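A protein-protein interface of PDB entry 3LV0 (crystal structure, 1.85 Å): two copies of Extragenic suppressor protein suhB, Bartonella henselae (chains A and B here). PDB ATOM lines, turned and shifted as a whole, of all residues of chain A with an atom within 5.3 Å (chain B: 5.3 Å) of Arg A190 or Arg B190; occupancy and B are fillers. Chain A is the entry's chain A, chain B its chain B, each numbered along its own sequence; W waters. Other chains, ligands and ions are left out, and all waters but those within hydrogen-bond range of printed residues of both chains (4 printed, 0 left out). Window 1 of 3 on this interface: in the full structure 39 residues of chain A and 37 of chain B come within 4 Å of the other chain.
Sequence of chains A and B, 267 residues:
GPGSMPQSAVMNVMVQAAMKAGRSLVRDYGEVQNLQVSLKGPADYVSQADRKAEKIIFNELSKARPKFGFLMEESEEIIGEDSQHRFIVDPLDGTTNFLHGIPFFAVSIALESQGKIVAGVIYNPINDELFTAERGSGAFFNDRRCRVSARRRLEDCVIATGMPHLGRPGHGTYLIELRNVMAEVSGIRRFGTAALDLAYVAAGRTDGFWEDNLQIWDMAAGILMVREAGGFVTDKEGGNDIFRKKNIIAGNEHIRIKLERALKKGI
Printed residues of chain A that touch a printed residue of chain B: Met A163, Ile A188, Arg A189, Arg A190, Phe A191 and Gly A192. Of the 11 printed residues of chain B, 6 touch a printed residue of chain A. Among the printed residues, 13 pairs touch across the chains.
Met B163 touches its own counterpart, Met A163. Met A163 touches Ile B188, and with the chains exchanged Ile A188 touches Met B163. Arg A189 touches Gly B192, and with the chains exchanged Gly A192 touches Arg B189. Arg B190 touches its own counterpart, Arg A190.
Water W1 lies within hydrogen-bond range of O of Gly A192 (2.7 Å) and NH2 of Arg B189 (3.0 Å). Water W2 bridges O of Gly B192 (2.7 Å) and NH2 of Arg A189 (3.1 Å). Water W3 lies within hydrogen-bond range of ND1 of His B165 (2.8 Å), NH2 of Arg B190 (3.0 Å) and N of Ile A188 (3.0 Å). Water W4 lies within hydrogen-bond range of ND1 of His A165 (2.8 Å), N of Ile B188 (3.0 Å) and NH2 of Arg A190 (3.1 Å).
The backbone carbonyl oxygen (O) of Ile A188 is in hydrogen-bond range of the guanidinium group (NE) of Arg B190 (3.1 Å). The backbone carbonyl oxygen (O) of Arg B190 is in hydrogen-bond range of the backbone NH (N) of Arg A190, at 2.9 Å. NE of Arg A190 lies within hydrogen-bond range of O of Ile B188 (3.2 Å).
Among the printed residues, pairs that only touch across the chains: Met A163 with Met B163 (3.8 Å), Met A163 with Ile B188 (3.8 Å), Ile A188 with Met B163 (3.8 Å), Arg A189 with Arg B190 (3.5 Å), Arg A189 with Phe B191 (3.4 Å), Arg A189 with Gly B192 (3.6 Å), Arg A190 with Arg B189 (3.4 Å), Phe A191 with Arg B189 (3.5 Å), Phe A191 with Phe B191 (3.9 Å) and Gly A192 with Arg B189 (3.7 Å).
Of chain B, only Ile B188 (3.2 Å), Arg B189 (3.4 Å) and Arg B190 (2.9 Å) come within 4 Å of Arg A190. Of chain A, only Ile A188, Arg A189 and Arg A190 come within 4 Å of Arg B190. Printed residues of chain B within 4 Å of Gly A192: Arg B189. Of the printed residues of chain B, Phe A191 touches Arg B189 (3.5 Å) and Phe B191 (3.9 Å). Of the printed residues of chain A, Phe B191 touches Arg A189 (3.4 Å) and Phe A191 (3.9 Å). Of the printed residues of chain A, Arg B189 touches Arg A190, Phe A191 and Gly A192. The nearest residue of chain B that does not touch Arg A190 is Phe B191 (4.5 Å). The nearest printed residue of chain B that does not touch Gly A192 is Ile B188 (5.8 Å).
O of Met B163 lies within hydrogen-bond range of NH2 of Arg B190, at 3.4 Å. O of Arg A189 sits at hydrogen-bond distance from N of Thr A161. The backbone NH of Thr B161 lies within hydrogen-bond range of the backbone carbonyl oxygen of Arg B189.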
ATOM      1  N   THR A 161       9.469  18.528  -6.398  1.00  0.00           N
ATOM      2  CA  THR A 161       8.583  19.658  -6.338  1.00  0.00           C
ATOM      3  C   THR A 161       7.245  19.260  -5.771  1.00  0.00           C
ATOM      4  O   THR A 161       6.882  18.085  -5.808  1.00  0.00           O
ATOM      5  CB  THR A 161       8.383  20.274  -7.736  1.00  0.00           C
ATOM      6  OG1 THR A 161       7.627  21.484  -7.599  1.00  0.00           O
ATOM      7  CG2 THR A 161       7.642  19.293  -8.670  1.00  0.00           C
ATOM      8  N   GLY A 162       6.517  20.247  -5.246  1.00  0.00           N
ATOM      9  CA  GLY A 162       5.144  20.024  -4.867  1.00  0.00           C
ATOM     10  C   GLY A 162       4.276  20.946  -5.688  1.00  0.00           C
ATOM     11  O   GLY A 162       4.658  22.060  -5.967  1.00  0.00           O
ATOM     12  N   MET A 163       3.085  20.501  -6.036  1.00  0.00           N
ATOM     13  CA  MET A 163       2.237  21.293  -6.920  1.00  0.00           C
ATOM     14  C   MET A 163       0.977  21.799  -6.238  1.00  0.00           C
ATOM     15  O   MET A 163       0.529  21.228  -5.237  1.00  0.00           O
ATOM     16  CB  MET A 163       1.844  20.464  -8.139  1.00  0.00           C
ATOM     17  CG  MET A 163       3.018  19.964  -8.947  1.00  0.00           C
ATOM     18  SD  MET A 163       2.434  18.997 -10.339  1.00  0.00           S
ATOM     19  CE  MET A 163       3.966  18.602 -11.195  1.00  0.00           C
ATOM     20  N   HIS A 165      -2.946  21.739  -7.002  1.00  0.00           N
ATOM     21  CA  HIS A 165      -3.863  21.113  -7.951  1.00  0.00           C
ATOM     22  C   HIS A 165      -5.243  21.653  -7.637  1.00  0.00           C
ATOM     23  O   HIS A 165      -5.355  22.733  -7.046  1.00  0.00           O
ATOM     24  CB  HIS A 165      -3.773  19.571  -7.924  1.00  0.00           C
ATOM     25  CG  HIS A 165      -3.715  18.994  -6.546  1.00  0.00           C
ATOM     26  ND1 HIS A 165      -2.577  18.404  -6.032  1.00  0.00           N
ATOM     27  CD2 HIS A 165      -4.643  18.951  -5.559  1.00  0.00           C
ATOM     28  CE1 HIS A 165      -2.810  18.014  -4.791  1.00  0.00           C
ATOM     29  NE2 HIS A 165      -4.057  18.330  -4.481  1.00  0.00           N
ATOM     30  N   ILE A 188      12.966  16.262 -12.887  1.00  0.00           N
ATOM     31  CA  ILE A 188      11.995  16.743 -11.903  1.00  0.00           C
ATOM     32  C   ILE A 188      11.259  15.530 -11.342  1.00  0.00           C
ATOM     33  O   ILE A 188      10.904  14.634 -12.089  1.00  0.00           O
ATOM     34  CB  ILE A 188      10.929  17.638 -12.573  1.00  0.00           C
ATOM     35  CG1 ILE A 188      11.596  18.856 -13.276  1.00  0.00           C
ATOM     36  CG2 ILE A 188       9.836  18.080 -11.540  1.00  0.00           C
ATOM     37  CD1 ILE A 188      12.072  19.904 -12.285  1.00  0.00           C
ATOM     38  N   ARG A 189      10.968  15.556 -10.053  1.00  0.00           N
ATOM     39  CA  ARG A 189      10.159  14.517  -9.439  1.00  0.00           C
ATOM     40  C   ARG A 189       9.014  15.144  -8.669  1.00  0.00           C
ATOM     41  O   ARG A 189       9.166  16.188  -8.013  1.00  0.00           O
ATOM     42  CB  ARG A 189      10.981  13.670  -8.463  1.00  0.00           C
ATOM     43  CG  ARG A 189      12.110  12.865  -9.104  1.00  0.00           C
ATOM     44  CD  ARG A 189      11.589  11.808 -10.061  1.00  0.00           C
ATOM     45  NE  ARG A 189      12.682  11.115 -10.759  1.00  0.00           N
ATOM     46  CZ  ARG A 189      13.239  11.470 -11.904  1.00  0.00           C
ATOM     47  NH1 ARG A 189      12.844  12.569 -12.580  1.00  0.00           N
ATOM     48  NH2 ARG A 189      14.221  10.701 -12.401  1.00  0.00           N
ATOM     49  N   ARG A 190       7.870  14.492  -8.730  1.00  0.00           N
ATOM     50  CA  ARG A 190       6.749  14.929  -7.895  1.00  0.00           C
ATOM     51  C   ARG A 190       6.187  13.676  -7.239  1.00  0.00           C
ATOM     52  O   ARG A 190       5.382  12.958  -7.828  1.00  0.00           O
ATOM     53  CB  ARG A 190       5.698  15.660  -8.733  1.00  0.00           C
ATOM     54  CG  ARG A 190       4.690  16.520  -7.913  1.00  0.00           C
ATOM     55  CD  ARG A 190       3.847  15.670  -6.973  1.00  0.00           C
ATOM     56  NE  ARG A 190       2.681  16.409  -6.468  1.00  0.00           N
ATOM     57  CZ  ARG A 190       2.624  17.000  -5.284  1.00  0.00           C
ATOM     58  NH1 ARG A 190       3.668  16.954  -4.445  1.00  0.00           N
ATOM     59  NH2 ARG A 190       1.510  17.637  -4.938  1.00  0.00           N
ATOM     60  N   PHE A 191       6.612  13.443  -5.996  1.00  0.00           N
ATOM     61  CA  PHE A 191       6.299  12.199  -5.299  1.00  0.00           C
ATOM     62  C   PHE A 191       4.980  12.208  -4.553  1.00  0.00           C
ATOM     63  O   PHE A 191       4.384  11.158  -4.412  1.00  0.00           O
ATOM     64  CB  PHE A 191       7.397  11.833  -4.291  1.00  0.00           C
ATOM     65  CG  PHE A 191       8.723  11.560  -4.928  1.00  0.00           C
ATOM     66  CD1 PHE A 191       8.845  10.576  -5.935  1.00  0.00           C
ATOM     67  CD2 PHE A 191       9.844  12.253  -4.513  1.00  0.00           C
ATOM     68  CE1 PHE A 191      10.099  10.327  -6.561  1.00  0.00           C
ATOM     69  CE2 PHE A 191      11.106  11.992  -5.102  1.00  0.00           C
ATOM     70  CZ  PHE A 191      11.225  11.025  -6.110  1.00  0.00           C
ATOM     71  N   GLY A 192       4.559  13.371  -4.096  1.00  0.00           N
ATOM     72  CA  GLY A 192       3.259  13.491  -3.406  1.00  0.00           C
ATOM     73  C   GLY A 192       3.397  13.500  -1.885  1.00  0.00           C
ATOM     74  O   GLY A 192       2.423  13.277  -1.176  1.00  0.00           O
ATOM     75  N   THR A 193       4.586  13.792  -1.415  1.00  0.00           N
ATOM     76  CA  THR A 193       4.757  13.928  -0.007  1.00  0.00           C
ATOM     77  C   THR A 193       5.366  15.284   0.154  1.00  0.00           C
ATOM     78  O   THR A 193       5.701  15.957  -0.817  1.00  0.00           O
ATOM     79  CB  THR A 193       5.693  12.837   0.485  1.00  0.00           C
ATOM     80  OG1 THR A 193       5.634  12.750   1.906  1.00  0.00           O
ATOM     81  CG2 THR A 193       7.117  13.173   0.057  1.00  0.00           C
ATOM     82  N   GLU A 211       8.228  24.086  -2.717  1.00  0.00           N
ATOM     83  CA  GLU A 211       6.764  23.929  -2.644  1.00  0.00           C
ATOM     84  C   GLU A 211       6.135  25.087  -1.888  1.00  0.00           C
ATOM     85  O   GLU A 211       6.792  25.740  -1.057  1.00  0.00           O
ATOM     86  CB  GLU A 211       6.338  22.598  -1.963  1.00  0.00           C
ATOM     87  CG  GLU A 211       4.776  22.379  -2.046  1.00  0.00           C
ATOM     88  CD  GLU A 211       4.324  20.948  -1.802  1.00  0.00           C
ATOM     89  OE1 GLU A 211       5.150  20.091  -1.429  1.00  0.00           O
ATOM     90  OE2 GLU A 211       3.128  20.675  -2.026  1.00  0.00           O
ATOM     91  N   THR B 161       2.702  11.262 -14.901  1.00  0.00           N
ATOM     92  CA  THR B 161       3.185  11.930 -16.077  1.00  0.00           C
ATOM     93  C   THR B 161       4.678  11.763 -16.206  1.00  0.00           C
ATOM     94  O   THR B 161       5.355  11.480 -15.231  1.00  0.00           O
ATOM     95  CB  THR B 161       2.805  13.425 -16.074  1.00  0.00           C
ATOM     96  OG1 THR B 161       3.081  13.962 -17.366  1.00  0.00           O
ATOM     97  CG2 THR B 161       3.616  14.253 -15.025  1.00  0.00           C
ATOM     98  N   GLY B 162       5.179  11.913 -17.422  1.00  0.00           N
ATOM     99  CA  GLY B 162       6.608  11.986 -17.627  1.00  0.00           C
ATOM    100  C   GLY B 162       6.914  13.360 -18.199  1.00  0.00           C
ATOM    101  O   GLY B 162       6.174  13.847 -19.028  1.00  0.00           O
ATOM    102  N   MET B 163       8.006  13.968 -17.765  1.00  0.00           N
ATOM    103  CA  MET B 163       8.365  15.321 -18.202  1.00  0.00           C
ATOM    104  C   MET B 163       9.613  15.357 -19.059  1.00  0.00           C
ATOM    105  O   MET B 163      10.579  14.614 -18.802  1.00  0.00           O
ATOM    106  CB  MET B 163       8.611  16.223 -17.002  1.00  0.00           C
ATOM    107  CG  MET B 163       7.465  16.336 -16.066  1.00  0.00           C
ATOM    108  SD  MET B 163       7.896  17.555 -14.831  1.00  0.00           S
ATOM    109  CE  MET B 163       6.530  17.403 -13.680  1.00  0.00           C
ATOM    110  N   HIS B 165      13.082  17.078 -19.774  1.00  0.00           N
ATOM    111  CA  HIS B 165      13.959  17.934 -18.998  1.00  0.00           C
ATOM    112  C   HIS B 165      15.060  18.364 -19.958  1.00  0.00           C
ATOM    113  O   HIS B 165      14.886  18.256 -21.181  1.00  0.00           O
ATOM    114  CB  HIS B 165      14.493  17.207 -17.745  1.00  0.00           C
ATOM    115  CG  HIS B 165      14.790  15.757 -17.969  1.00  0.00           C
ATOM    116  ND1 HIS B 165      14.098  14.748 -17.330  1.00  0.00           N
ATOM    117  CD2 HIS B 165      15.682  15.144 -18.785  1.00  0.00           C
ATOM    118  CE1 HIS B 165      14.562  13.577 -17.730  1.00  0.00           C
ATOM    119  NE2 HIS B 165      15.523  13.789 -18.613  1.00  0.00           N
ATOM    120  N   ILE B 188      -1.165  15.202  -9.395  1.00  0.00           N
ATOM    121  CA  ILE B 188      -0.246  14.804 -10.460  1.00  0.00           C
ATOM    122  C   ILE B 188       0.966  14.127  -9.800  1.00  0.00           C
ATOM    123  O   ILE B 188       1.419  14.603  -8.758  1.00  0.00           O
ATOM    124  CB  ILE B 188       0.261  16.065 -11.218  1.00  0.00           C
ATOM    125  CG1 ILE B 188      -0.929  16.769 -11.930  1.00  0.00           C
ATOM    126  CG2 ILE B 188       1.361  15.686 -12.228  1.00  0.00           C
ATOM    127  CD1 ILE B 188      -1.335  16.026 -13.168  1.00  0.00           C
ATOM    128  N   ARG B 189       1.484  13.071 -10.411  1.00  0.00           N
ATOM    129  CA  ARG B 189       2.718  12.428  -9.939  1.00  0.00           C
ATOM    130  C   ARG B 189       3.737  12.281 -11.050  1.00  0.00           C
ATOM    131  O   ARG B 189       3.379  12.015 -12.197  1.00  0.00           O
ATOM    132  CB  ARG B 189       2.404  11.025  -9.380  1.00  0.00           C
ATOM    133  CG  ARG B 189       1.428  11.083  -8.193  1.00  0.00           C
ATOM    134  CD  ARG B 189       2.085  11.690  -6.963  1.00  0.00           C
ATOM    135  NE  ARG B 189       1.166  11.706  -5.811  1.00  0.00           N
ATOM    136  CZ  ARG B 189       0.318  12.677  -5.491  1.00  0.00           C
ATOM    137  NH1 ARG B 189       0.197  13.790  -6.231  1.00  0.00           N
ATOM    138  NH2 ARG B 189      -0.443  12.538  -4.403  1.00  0.00           N
ATOM    139  N   ARG B 190       5.012  12.385 -10.689  1.00  0.00           N
ATOM    140  CA  ARG B 190       6.082  12.217 -11.671  1.00  0.00           C
ATOM    141  C   ARG B 190       7.120  11.410 -10.901  1.00  0.00           C
ATOM    142  O   ARG B 190       7.951  11.965 -10.173  1.00  0.00           O
ATOM    143  CB  ARG B 190       6.652  13.591 -12.106  1.00  0.00           C
ATOM    144  CG  ARG B 190       7.491  13.609 -13.431  1.00  0.00           C
ATOM    145  CD  ARG B 190       8.698  12.712 -13.299  1.00  0.00           C
ATOM    146  NE  ARG B 190       9.675  12.910 -14.375  1.00  0.00           N
ATOM    147  CZ  ARG B 190       9.908  12.037 -15.350  1.00  0.00           C
ATOM    148  NH1 ARG B 190       9.228  10.892 -15.402  1.00  0.00           N
ATOM    149  NH2 ARG B 190      10.845  12.309 -16.265  1.00  0.00           N
ATOM    150  N   PHE B 191       7.057  10.104 -11.059  1.00  0.00           N
ATOM    151  CA  PHE B 191       7.898   9.223 -10.242  1.00  0.00           C
ATOM    152  C   PHE B 191       9.276   8.988 -10.853  1.00  0.00           C
ATOM    153  O   PHE B 191      10.220   8.707 -10.107  1.00  0.00           O
ATOM    154  CB  PHE B 191       7.227   7.853 -10.053  1.00  0.00           C
ATOM    155  CG  PHE B 191       5.910   7.921  -9.335  1.00  0.00           C
ATOM    156  CD1 PHE B 191       5.829   8.496  -8.074  1.00  0.00           C
ATOM    157  CD2 PHE B 191       4.755   7.420  -9.922  1.00  0.00           C
ATOM    158  CE1 PHE B 191       4.594   8.583  -7.394  1.00  0.00           C
ATOM    159  CE2 PHE B 191       3.508   7.503  -9.239  1.00  0.00           C
ATOM    160  CZ  PHE B 191       3.457   8.066  -7.989  1.00  0.00           C
ATOM    161  N   GLY B 192       9.374   9.080 -12.172  1.00  0.00           N
ATOM    162  CA  GLY B 192      10.691   8.939 -12.842  1.00  0.00           C
ATOM    163  C   GLY B 192      10.863   7.601 -13.541  1.00  0.00           C
ATOM    164  O   GLY B 192      11.976   7.237 -13.912  1.00  0.00           O
ATOM    165  N   THR B 193       9.768   6.895 -13.709  1.00  0.00           N
ATOM    166  CA  THR B 193       9.827   5.664 -14.430  1.00  0.00           C
ATOM    167  C   THR B 193       8.854   5.842 -15.565  1.00  0.00           C
ATOM    168  O   THR B 193       8.125   6.831 -15.627  1.00  0.00           O
ATOM    169  CB  THR B 193       9.396   4.536 -13.500  1.00  0.00           C
ATOM    170  OG1 THR B 193       9.756   3.267 -14.055  1.00  0.00           O
ATOM    171  CG2 THR B 193       7.918   4.599 -13.338  1.00  0.00           C
ATOM    172  N   GLU B 211       2.846  10.519 -21.510  1.00  0.00           N
ATOM    173  CA  GLU B 211       4.261  10.901 -21.705  1.00  0.00           C
ATOM    174  C   GLU B 211       4.595  10.833 -23.177  1.00  0.00           C
ATOM    175  O   GLU B 211       3.915  10.134 -23.947  1.00  0.00           O
ATOM    176  CB  GLU B 211       5.265  10.001 -20.922  1.00  0.00           C
ATOM    177  CG  GLU B 211       6.721  10.590 -20.962  1.00  0.00           C
ATOM    178  CD  GLU B 211       7.696   9.931 -20.010  1.00  0.00           C
ATOM    179  OE1 GLU B 211       7.285   9.041 -19.236  1.00  0.00           O
ATOM    180  OE2 GLU B 211       8.882  10.334 -20.023  1.00  0.00           O
HETATM  181  O   HOH W   1       0.020  12.090  -1.468  1.00  0.00           O
HETATM  182  O   HOH W   2      14.553   7.760 -13.228  1.00  0.00           O
HETATM  183  O   HOH W   3      12.054  14.910 -15.413  1.00  0.00           O
HETATM  184  O   HOH W   4      -0.390  17.179  -7.325  1.00  0.00           O
